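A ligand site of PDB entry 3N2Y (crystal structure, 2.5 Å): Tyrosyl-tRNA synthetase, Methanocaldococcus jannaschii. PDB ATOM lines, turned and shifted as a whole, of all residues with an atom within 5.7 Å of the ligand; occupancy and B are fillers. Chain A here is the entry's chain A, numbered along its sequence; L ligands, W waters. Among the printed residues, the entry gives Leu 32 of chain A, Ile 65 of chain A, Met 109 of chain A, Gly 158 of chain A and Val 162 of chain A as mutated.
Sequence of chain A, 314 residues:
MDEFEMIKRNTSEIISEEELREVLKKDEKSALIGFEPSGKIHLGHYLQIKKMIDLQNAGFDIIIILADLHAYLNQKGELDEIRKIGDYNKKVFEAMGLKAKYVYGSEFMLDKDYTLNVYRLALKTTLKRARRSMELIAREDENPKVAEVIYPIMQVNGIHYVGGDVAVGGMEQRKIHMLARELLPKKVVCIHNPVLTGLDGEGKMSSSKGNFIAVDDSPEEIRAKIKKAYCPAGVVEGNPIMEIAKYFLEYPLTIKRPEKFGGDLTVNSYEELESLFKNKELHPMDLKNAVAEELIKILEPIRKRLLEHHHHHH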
ATOM      1  N   LEU A  32      31.389  17.777 -11.740  1.00  0.00           N
ATOM      2  CA  LEU A  32      30.725  19.022 -11.371  1.00  0.00           C
ATOM      3  C   LEU A  32      31.588  19.929 -10.516  1.00  0.00           C
ATOM      4  O   LEU A  32      32.539  19.486  -9.874  1.00  0.00           O
ATOM      5  CB  LEU A  32      29.347  18.769 -10.729  1.00  0.00           C
ATOM      6  CG  LEU A  32      29.105  18.371  -9.257  1.00  0.00           C
ATOM      7  CD1 LEU A  32      29.713  17.016  -8.907  1.00  0.00           C
ATOM      8  CD2 LEU A  32      29.563  19.424  -8.266  1.00  0.00           C
ATOM      9  N   ILE A  33      31.235  21.210 -10.524  1.00  0.00           N
ATOM     10  CA  ILE A  33      31.795  22.209  -9.630  1.00  0.00           C
ATOM     11  C   ILE A  33      30.719  23.251  -9.436  1.00  0.00           C
ATOM     12  O   ILE A  33      29.886  23.454 -10.322  1.00  0.00           O
ATOM     13  CB  ILE A  33      33.122  22.840 -10.187  1.00  0.00           C
ATOM     14  CG1 ILE A  33      33.716  23.836  -9.190  1.00  0.00           C
ATOM     15  CG2 ILE A  33      32.902  23.517 -11.547  1.00  0.00           C
ATOM     16  CD1 ILE A  33      35.190  24.155  -9.431  1.00  0.00           C
ATOM     17  N   GLY A  34      30.720  23.896  -8.277  1.00  0.00           N
ATOM     18  CA  GLY A  34      29.777  24.960  -8.012  1.00  0.00           C
ATOM     19  C   GLY A  34      30.474  26.228  -7.601  1.00  0.00           C
ATOM     20  O   GLY A  34      31.567  26.199  -7.031  1.00  0.00           O
ATOM     21  N   PHE A  35      29.861  27.352  -7.918  1.00  0.00           N
ATOM     22  CA  PHE A  35      30.435  28.635  -7.583  1.00  0.00           C
ATOM     23  C   PHE A  35      29.390  29.551  -6.991  1.00  0.00           C
ATOM     24  O   PHE A  35      28.319  29.732  -7.571  1.00  0.00           O
ATOM     25  CB  PHE A  35      31.030  29.321  -8.813  1.00  0.00           C
ATOM     26  CG  PHE A  35      32.298  28.708  -9.316  1.00  0.00           C
ATOM     27  CD1 PHE A  35      32.288  27.890 -10.437  1.00  0.00           C
ATOM     28  CD2 PHE A  35      33.506  28.960  -8.666  1.00  0.00           C
ATOM     29  CE1 PHE A  35      33.466  27.311 -10.906  1.00  0.00           C
ATOM     30  CE2 PHE A  35      34.691  28.394  -9.133  1.00  0.00           C
ATOM     31  CZ  PHE A  35      34.667  27.575 -10.251  1.00  0.00           C
ATOM     32  N   GLU A  36      29.716  30.103  -5.832  1.00  0.00           N
ATOM     33  CA  GLU A  36      29.025  31.287  -5.359  1.00  0.00           C
ATOM     34  C   GLU A  36      29.414  32.418  -6.305  1.00  0.00           C
ATOM     35  O   GLU A  36      30.612  32.737  -6.435  1.00  0.00           O
ATOM     36  CB  GLU A  36      29.458  31.631  -3.938  1.00  0.00           C
ATOM     37  CG  GLU A  36      28.747  30.832  -2.876  1.00  0.00           C
ATOM     38  CD  GLU A  36      29.087  31.339  -1.500  1.00  0.00           C
ATOM     39  OE1 GLU A  36      29.072  32.563  -1.294  1.00  0.00           O
ATOM     40  OE2 GLU A  36      29.391  30.504  -0.618  1.00  0.00           O
ATOM     41  N   ILE A  65      27.544  24.539 -11.520  1.00  0.00           N
ATOM     42  CA  ILE A  65      26.424  25.025 -10.734  1.00  0.00           C
ATOM     43  C   ILE A  65      26.697  26.463 -10.361  1.00  0.00           C
ATOM     44  O   ILE A  65      27.658  26.760  -9.666  1.00  0.00           O
ATOM     45  CB  ILE A  65      26.122  24.151  -9.476  1.00  0.00           C
ATOM     46  CG1 ILE A  65      25.603  22.760  -9.872  1.00  0.00           C
ATOM     47  CG2 ILE A  65      25.102  24.838  -8.568  1.00  0.00           C
ATOM     48  CD1 ILE A  65      26.708  21.698 -10.041  1.00  0.00           C
ATOM     49  N   ALA A  67      25.737  28.766  -8.033  1.00  0.00           N
ATOM     50  CA  ALA A  67      25.095  28.549  -6.741  1.00  0.00           C
ATOM     51  C   ALA A  67      24.495  29.807  -6.131  1.00  0.00           C
ATOM     52  O   ALA A  67      24.992  30.332  -5.113  1.00  0.00           O
ATOM     53  CB  ALA A  67      26.076  27.911  -5.776  1.00  0.00           C
ATOM     54  N   HIS A  70      23.074  29.137  -2.492  1.00  0.00           N
ATOM     55  CA  HIS A  70      24.199  29.054  -1.571  1.00  0.00           C
ATOM     56  C   HIS A  70      24.775  30.431  -1.221  1.00  0.00           C
ATOM     57  O   HIS A  70      25.102  30.698  -0.064  1.00  0.00           O
ATOM     58  CB  HIS A  70      25.268  28.125  -2.116  1.00  0.00           C
ATOM     59  CG  HIS A  70      24.934  26.675  -1.992  1.00  0.00           C
ATOM     60  ND1 HIS A  70      24.175  26.011  -2.929  1.00  0.00           N
ATOM     61  CD2 HIS A  70      25.256  25.763  -1.049  1.00  0.00           C
ATOM     62  CE1 HIS A  70      24.044  24.742  -2.562  1.00  0.00           C
ATOM     63  NE2 HIS A  70      24.689  24.566  -1.429  1.00  0.00           N
ATOM     64  N   PHE A 108      16.497  23.704  -9.209  1.00  0.00           N
ATOM     65  CA  PHE A 108      16.177  22.356  -8.729  1.00  0.00           C
ATOM     66  C   PHE A 108      16.307  22.202  -7.203  1.00  0.00           C
ATOM     67  O   PHE A 108      15.970  21.153  -6.654  1.00  0.00           O
ATOM     68  CB  PHE A 108      17.065  21.332  -9.436  1.00  0.00           C
ATOM     69  CG  PHE A 108      18.536  21.457  -9.101  1.00  0.00           C
ATOM     70  CD1 PHE A 108      19.050  20.869  -7.953  1.00  0.00           C
ATOM     71  CD2 PHE A 108      19.395  22.147  -9.949  1.00  0.00           C
ATOM     72  CE1 PHE A 108      20.418  20.978  -7.632  1.00  0.00           C
ATOM     73  CE2 PHE A 108      20.753  22.271  -9.640  1.00  0.00           C
ATOM     74  CZ  PHE A 108      21.265  21.673  -8.470  1.00  0.00           C
ATOM     75  N   MET A 109      16.802  23.235  -6.537  1.00  0.00           N
ATOM     76  CA  MET A 109      17.096  23.172  -5.105  1.00  0.00           C
ATOM     77  C   MET A 109      15.905  23.530  -4.206  1.00  0.00           C
ATOM     78  O   MET A 109      16.056  23.611  -2.979  1.00  0.00           O
ATOM     79  CB  MET A 109      18.302  24.046  -4.756  1.00  0.00           C
ATOM     80  CG  MET A 109      19.647  23.368  -4.982  1.00  0.00           C
ATOM     81  SD  MET A 109      21.087  24.406  -4.665  1.00  0.00           S
ATOM     82  CE  MET A 109      22.392  23.260  -5.112  1.00  0.00           C
ATOM     83  N   TYR A 114      13.583  17.462  -3.075  1.00  0.00           N
ATOM     84  CA  TYR A 114      14.922  17.965  -2.827  1.00  0.00           C
ATOM     85  C   TYR A 114      14.989  18.504  -1.394  1.00  0.00           C
ATOM     86  O   TYR A 114      15.892  18.138  -0.629  1.00  0.00           O
ATOM     87  CB  TYR A 114      15.296  19.080  -3.824  1.00  0.00           C
ATOM     88  CG  TYR A 114      16.736  19.516  -3.689  1.00  0.00           C
ATOM     89  CD1 TYR A 114      17.709  19.036  -4.565  1.00  0.00           C
ATOM     90  CD2 TYR A 114      17.132  20.397  -2.678  1.00  0.00           C
ATOM     91  CE1 TYR A 114      19.042  19.433  -4.438  1.00  0.00           C
ATOM     92  CE2 TYR A 114      18.460  20.794  -2.537  1.00  0.00           C
ATOM     93  CZ  TYR A 114      19.405  20.305  -3.417  1.00  0.00           C
ATOM     94  OH  TYR A 114      20.717  20.689  -3.288  1.00  0.00           O
ATOM     95  N   ILE A 137      34.571  28.606   4.353  1.00  0.00           N
ATOM     96  CA  ILE A 137      33.600  29.017   3.352  1.00  0.00           C
ATOM     97  C   ILE A 137      32.683  30.131   3.858  1.00  0.00           C
ATOM     98  O   ILE A 137      32.374  31.067   3.114  1.00  0.00           O
ATOM     99  CB  ILE A 137      32.743  27.806   2.874  1.00  0.00           C
ATOM    100  CG1 ILE A 137      33.619  26.786   2.140  1.00  0.00           C
ATOM    101  CG2 ILE A 137      31.577  28.259   2.004  1.00  0.00           C
ATOM    102  CD1 ILE A 137      32.990  25.406   2.020  1.00  0.00           C
ATOM    103  N   TYR A 151      23.585  25.390   4.478  1.00  0.00           N
ATOM    104  CA  TYR A 151      24.473  25.444   3.317  1.00  0.00           C
ATOM    105  C   TYR A 151      25.162  24.088   2.997  1.00  0.00           C
ATOM    106  O   TYR A 151      25.026  23.590   1.876  1.00  0.00           O
ATOM    107  CB  TYR A 151      25.509  26.552   3.546  1.00  0.00           C
ATOM    108  CG  TYR A 151      26.437  26.889   2.407  1.00  0.00           C
ATOM    109  CD1 TYR A 151      26.306  28.100   1.729  1.00  0.00           C
ATOM    110  CD2 TYR A 151      27.466  26.018   2.026  1.00  0.00           C
ATOM    111  CE1 TYR A 151      27.172  28.437   0.688  1.00  0.00           C
ATOM    112  CE2 TYR A 151      28.331  26.349   0.978  1.00  0.00           C
ATOM    113  CZ  TYR A 151      28.175  27.570   0.320  1.00  0.00           C
ATOM    114  OH  TYR A 151      28.999  27.928  -0.706  1.00  0.00           O
ATOM    115  N   MET A 154      22.928  21.291   1.840  1.00  0.00           N
ATOM    116  CA  MET A 154      22.338  21.602   0.550  1.00  0.00           C
ATOM    117  C   MET A 154      23.307  21.368  -0.605  1.00  0.00           C
ATOM    118  O   MET A 154      22.888  20.975  -1.688  1.00  0.00           O
ATOM    119  CB  MET A 154      21.796  23.021   0.515  1.00  0.00           C
ATOM    120  CG  MET A 154      20.300  23.067   0.356  1.00  0.00           C
ATOM    121  SD  MET A 154      19.642  24.735   0.183  1.00  0.00           S
ATOM    122  CE  MET A 154      20.823  25.429  -0.993  1.00  0.00           C
ATOM    123  N   GLN A 155      24.597  21.588  -0.353  1.00  0.00           N
ATOM    124  CA  GLN A 155      25.623  21.241  -1.319  1.00  0.00           C
ATOM    125  C   GLN A 155      25.722  19.725  -1.503  1.00  0.00           C
ATOM    126  O   GLN A 155      25.757  19.241  -2.630  1.00  0.00           O
ATOM    127  CB  GLN A 155      26.972  21.824  -0.904  1.00  0.00           C
ATOM    128  CG  GLN A 155      28.091  21.633  -1.931  1.00  0.00           C
ATOM    129  CD  GLN A 155      29.285  22.508  -1.647  1.00  0.00           C
ATOM    130  OE1 GLN A 155      29.181  23.525  -0.949  1.00  0.00           O
ATOM    131  NE2 GLN A 155      30.449  22.128  -2.186  1.00  0.00           N
ATOM    132  N   ASN A 157      23.383  17.463  -0.906  1.00  0.00           N
ATOM    133  CA  ASN A 157      22.179  17.067  -1.634  1.00  0.00           C
ATOM    134  C   ASN A 157      22.249  17.414  -3.121  1.00  0.00           C
ATOM    135  O   ASN A 157      21.834  16.628  -3.960  1.00  0.00           O
ATOM    136  CB  ASN A 157      20.913  17.658  -1.009  1.00  0.00           C
ATOM    137  CG  ASN A 157      19.670  16.862  -1.365  1.00  0.00           C
ATOM    138  OD1 ASN A 157      19.641  15.640  -1.256  1.00  0.00           O
ATOM    139  ND2 ASN A 157      18.636  17.559  -1.802  1.00  0.00           N
ATOM    140  N   GLY A 158      22.773  18.604  -3.419  1.00  0.00           N
ATOM    141  CA  GLY A 158      23.067  19.024  -4.797  1.00  0.00           C
ATOM    142  C   GLY A 158      23.968  18.018  -5.507  1.00  0.00           C
ATOM    143  O   GLY A 158      23.628  17.506  -6.566  1.00  0.00           O
ATOM    144  N   ILE A 159      25.110  17.729  -4.898  1.00  0.00           N
ATOM    145  CA  ILE A 159      26.024  16.681  -5.354  1.00  0.00           C
ATOM    146  C   ILE A 159      25.279  15.384  -5.683  1.00  0.00           C
ATOM    147  O   ILE A 159      25.496  14.781  -6.734  1.00  0.00           O
ATOM    148  CB  ILE A 159      27.159  16.437  -4.327  1.00  0.00           C
ATOM    149  CG1 ILE A 159      28.071  17.671  -4.251  1.00  0.00           C
ATOM    150  CG2 ILE A 159      27.958  15.188  -4.670  1.00  0.00           C
ATOM    151  CD1 ILE A 159      28.994  17.667  -3.059  1.00  0.00           C
ATOM    152  N   VAL A 162      22.566  16.121  -8.799  1.00  0.00           N
ATOM    153  CA  VAL A 162      23.244  16.254 -10.091  1.00  0.00           C
ATOM    154  C   VAL A 162      23.750  14.911 -10.620  1.00  0.00           C
ATOM    155  O   VAL A 162      23.715  14.666 -11.831  1.00  0.00           O
ATOM    156  CB  VAL A 162      24.413  17.267 -10.007  1.00  0.00           C
ATOM    157  CG1 VAL A 162      25.269  17.232 -11.261  1.00  0.00           C
ATOM    158  CG2 VAL A 162      23.871  18.672  -9.771  1.00  0.00           C
ATOM    159  N   GLU A 172      39.018  24.334   0.463  1.00  0.00           N
ATOM    160  CA  GLU A 172      37.966  24.809   1.379  1.00  0.00           C
ATOM    161  C   GLU A 172      36.705  23.931   1.364  1.00  0.00           C
ATOM    162  O   GLU A 172      35.931  23.927   2.302  1.00  0.00           O
ATOM    163  CB  GLU A 172      37.543  26.269   1.062  1.00  0.00           C
ATOM    164  CG  GLU A 172      38.554  27.140   0.295  1.00  0.00           C
ATOM    165  CD  GLU A 172      38.555  26.853  -1.210  1.00  0.00           C
ATOM    166  OE1 GLU A 172      37.481  26.547  -1.780  1.00  0.00           O
ATOM    167  OE2 GLU A 172      39.643  26.938  -1.811  1.00  0.00           O
ATOM    168  N   GLN A 173      36.522  23.193   0.277  1.00  0.00           N
ATOM    169  CA  GLN A 173      35.324  22.362   0.073  1.00  0.00           C
ATOM    170  C   GLN A 173      35.531  20.939   0.565  1.00  0.00           C
ATOM    171  O   GLN A 173      34.624  20.124   0.496  1.00  0.00           O
ATOM    172  CB  GLN A 173      34.963  22.317  -1.419  1.00  0.00           C
ATOM    173  CG  GLN A 173      35.120  23.630  -2.176  1.00  0.00           C
ATOM    174  CD  GLN A 173      34.026  24.613  -1.866  1.00  0.00           C
ATOM    175  OE1 GLN A 173      32.841  24.290  -1.942  1.00  0.00           O
ATOM    176  NE2 GLN A 173      34.413  25.839  -1.514  1.00  0.00           N
ATOM    177  N   ILE A 176      33.024  19.391   3.402  1.00  0.00           N
ATOM    178  CA  ILE A 176      31.709  19.161   2.811  1.00  0.00           C
ATOM    179  C   ILE A 176      31.724  17.960   1.859  1.00  0.00           C
ATOM    180  O   ILE A 176      30.737  17.257   1.721  1.00  0.00           O
ATOM    181  CB  ILE A 176      31.166  20.419   2.064  1.00  0.00           C
ATOM    182  CG1 ILE A 176      30.938  21.568   3.045  1.00  0.00           C
ATOM    183  CG2 ILE A 176      29.885  20.095   1.299  1.00  0.00           C
ATOM    184  CD1 ILE A 176      30.394  22.838   2.419  1.00  0.00           C
HETATM  185  C1  LIG L   1      31.094  26.419  -2.754  1.00  0.00           C
HETATM  186  N1  LIG L   1      30.483  25.929  -1.527  1.00  0.00           N
HETATM  187  O1  LIG L   1      31.919  28.535  -3.378  1.00  0.00           O
HETATM  188  C2  LIG L   1      30.005  26.749  -3.766  1.00  0.00           C
HETATM  189  N2  LIG L   1      26.998  22.263  -5.577  1.00  0.00           N
HETATM  190  O2  LIG L   1      32.409  27.809  -1.348  1.00  0.00           O
HETATM  191  C3  LIG L   1      29.258  25.519  -4.241  1.00  0.00           C
HETATM  192  N3  LIG L   1      27.566  21.059  -5.982  1.00  0.00           N
HETATM  193  C4  LIG L   1      27.868  25.584  -4.325  1.00  0.00           C
HETATM  194  N4  LIG L   1      25.335  20.997  -6.188  1.00  0.00           N
HETATM  195  C5  LIG L   1      27.128  24.501  -4.779  1.00  0.00           C
HETATM  196  N5  LIG L   1      25.606  22.285  -5.692  1.00  0.00           N
HETATM  197  C6  LIG L   1      27.727  23.302  -5.165  1.00  0.00           C
HETATM  198  C7  LIG L   1      26.493  20.301  -6.338  1.00  0.00           C
HETATM  199  C8  LIG L   1      29.131  23.268  -5.069  1.00  0.00           C
HETATM  200  C9  LIG L   1      29.902  24.342  -4.612  1.00  0.00           C
HETATM  201  C10 LIG L   1      31.869  27.675  -2.473  1.00  0.00           C
HETATM  202  O   HOH W   1      32.479  22.691  -6.211  1.00  0.00           O
HETATM  203  O   HOH W   2      30.824  20.343  -4.701  1.00  0.00           O
HETATM  204  O   HOH W   3      33.107  30.825  -0.813  1.00  0.00           O
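OE1 of Gln 155 is in hydrogen-bond range of N1 of the ligand. NE2 of Gln 173 is in hydrogen-bond range of O2 of the ligand. OH of Tyr 151 sits at hydrogen-bond distance from N1 of the ligand (2.6 Å).
N of Ala 67 is in hydrogen-bond range of O of Phe 35, 2.8 Å away. The backbone carbonyl oxygen (O) of Tyr 151 is in hydrogen-bond range of a ring nitrogen (NE2) of His 70, at 3.5 Å. OE1 of Gln 173 is in hydrogen-bond range of NE2 of Gln 155. N of Ile 65 is in hydrogen-bond range of O of Ile 33, 2.8 Å away. OE1 of Glu 172 lies within hydrogen-bond range of NE2 of Gln 173, 3.2 Å away. The side-chain hydroxyl of Tyr 151 is in hydrogen-bond range of the side-chain carboxylate of Glu 36 (2.6 Å). The backbone NH (N) of Phe 35 is in hydrogen-bond range of the backbone carbonyl oxygen (O) of Ile 65 (2.9 Å). N of Gly 158 is in hydrogen-bond range of OH of Tyr 114.
Merely in contact with the ligand: Leu 32 (3.4 Å), Gly 34 (3.5 Å), Glu 36 (3.7 Å), Ile 65 (3.9 Å), Ala 67 (3.3 Å), His 70 (3.8 Å), Met 109 (3.4 Å), Ile 137 (3.5 Å), Gly 158 (3.3 Å) and Ile 159 (3.3 Å). Of the 22 residues printed, 13 come within 4 Å of the ligand. The nearest printed residue that does not touch the ligand is Phe 35 (4.2 Å).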
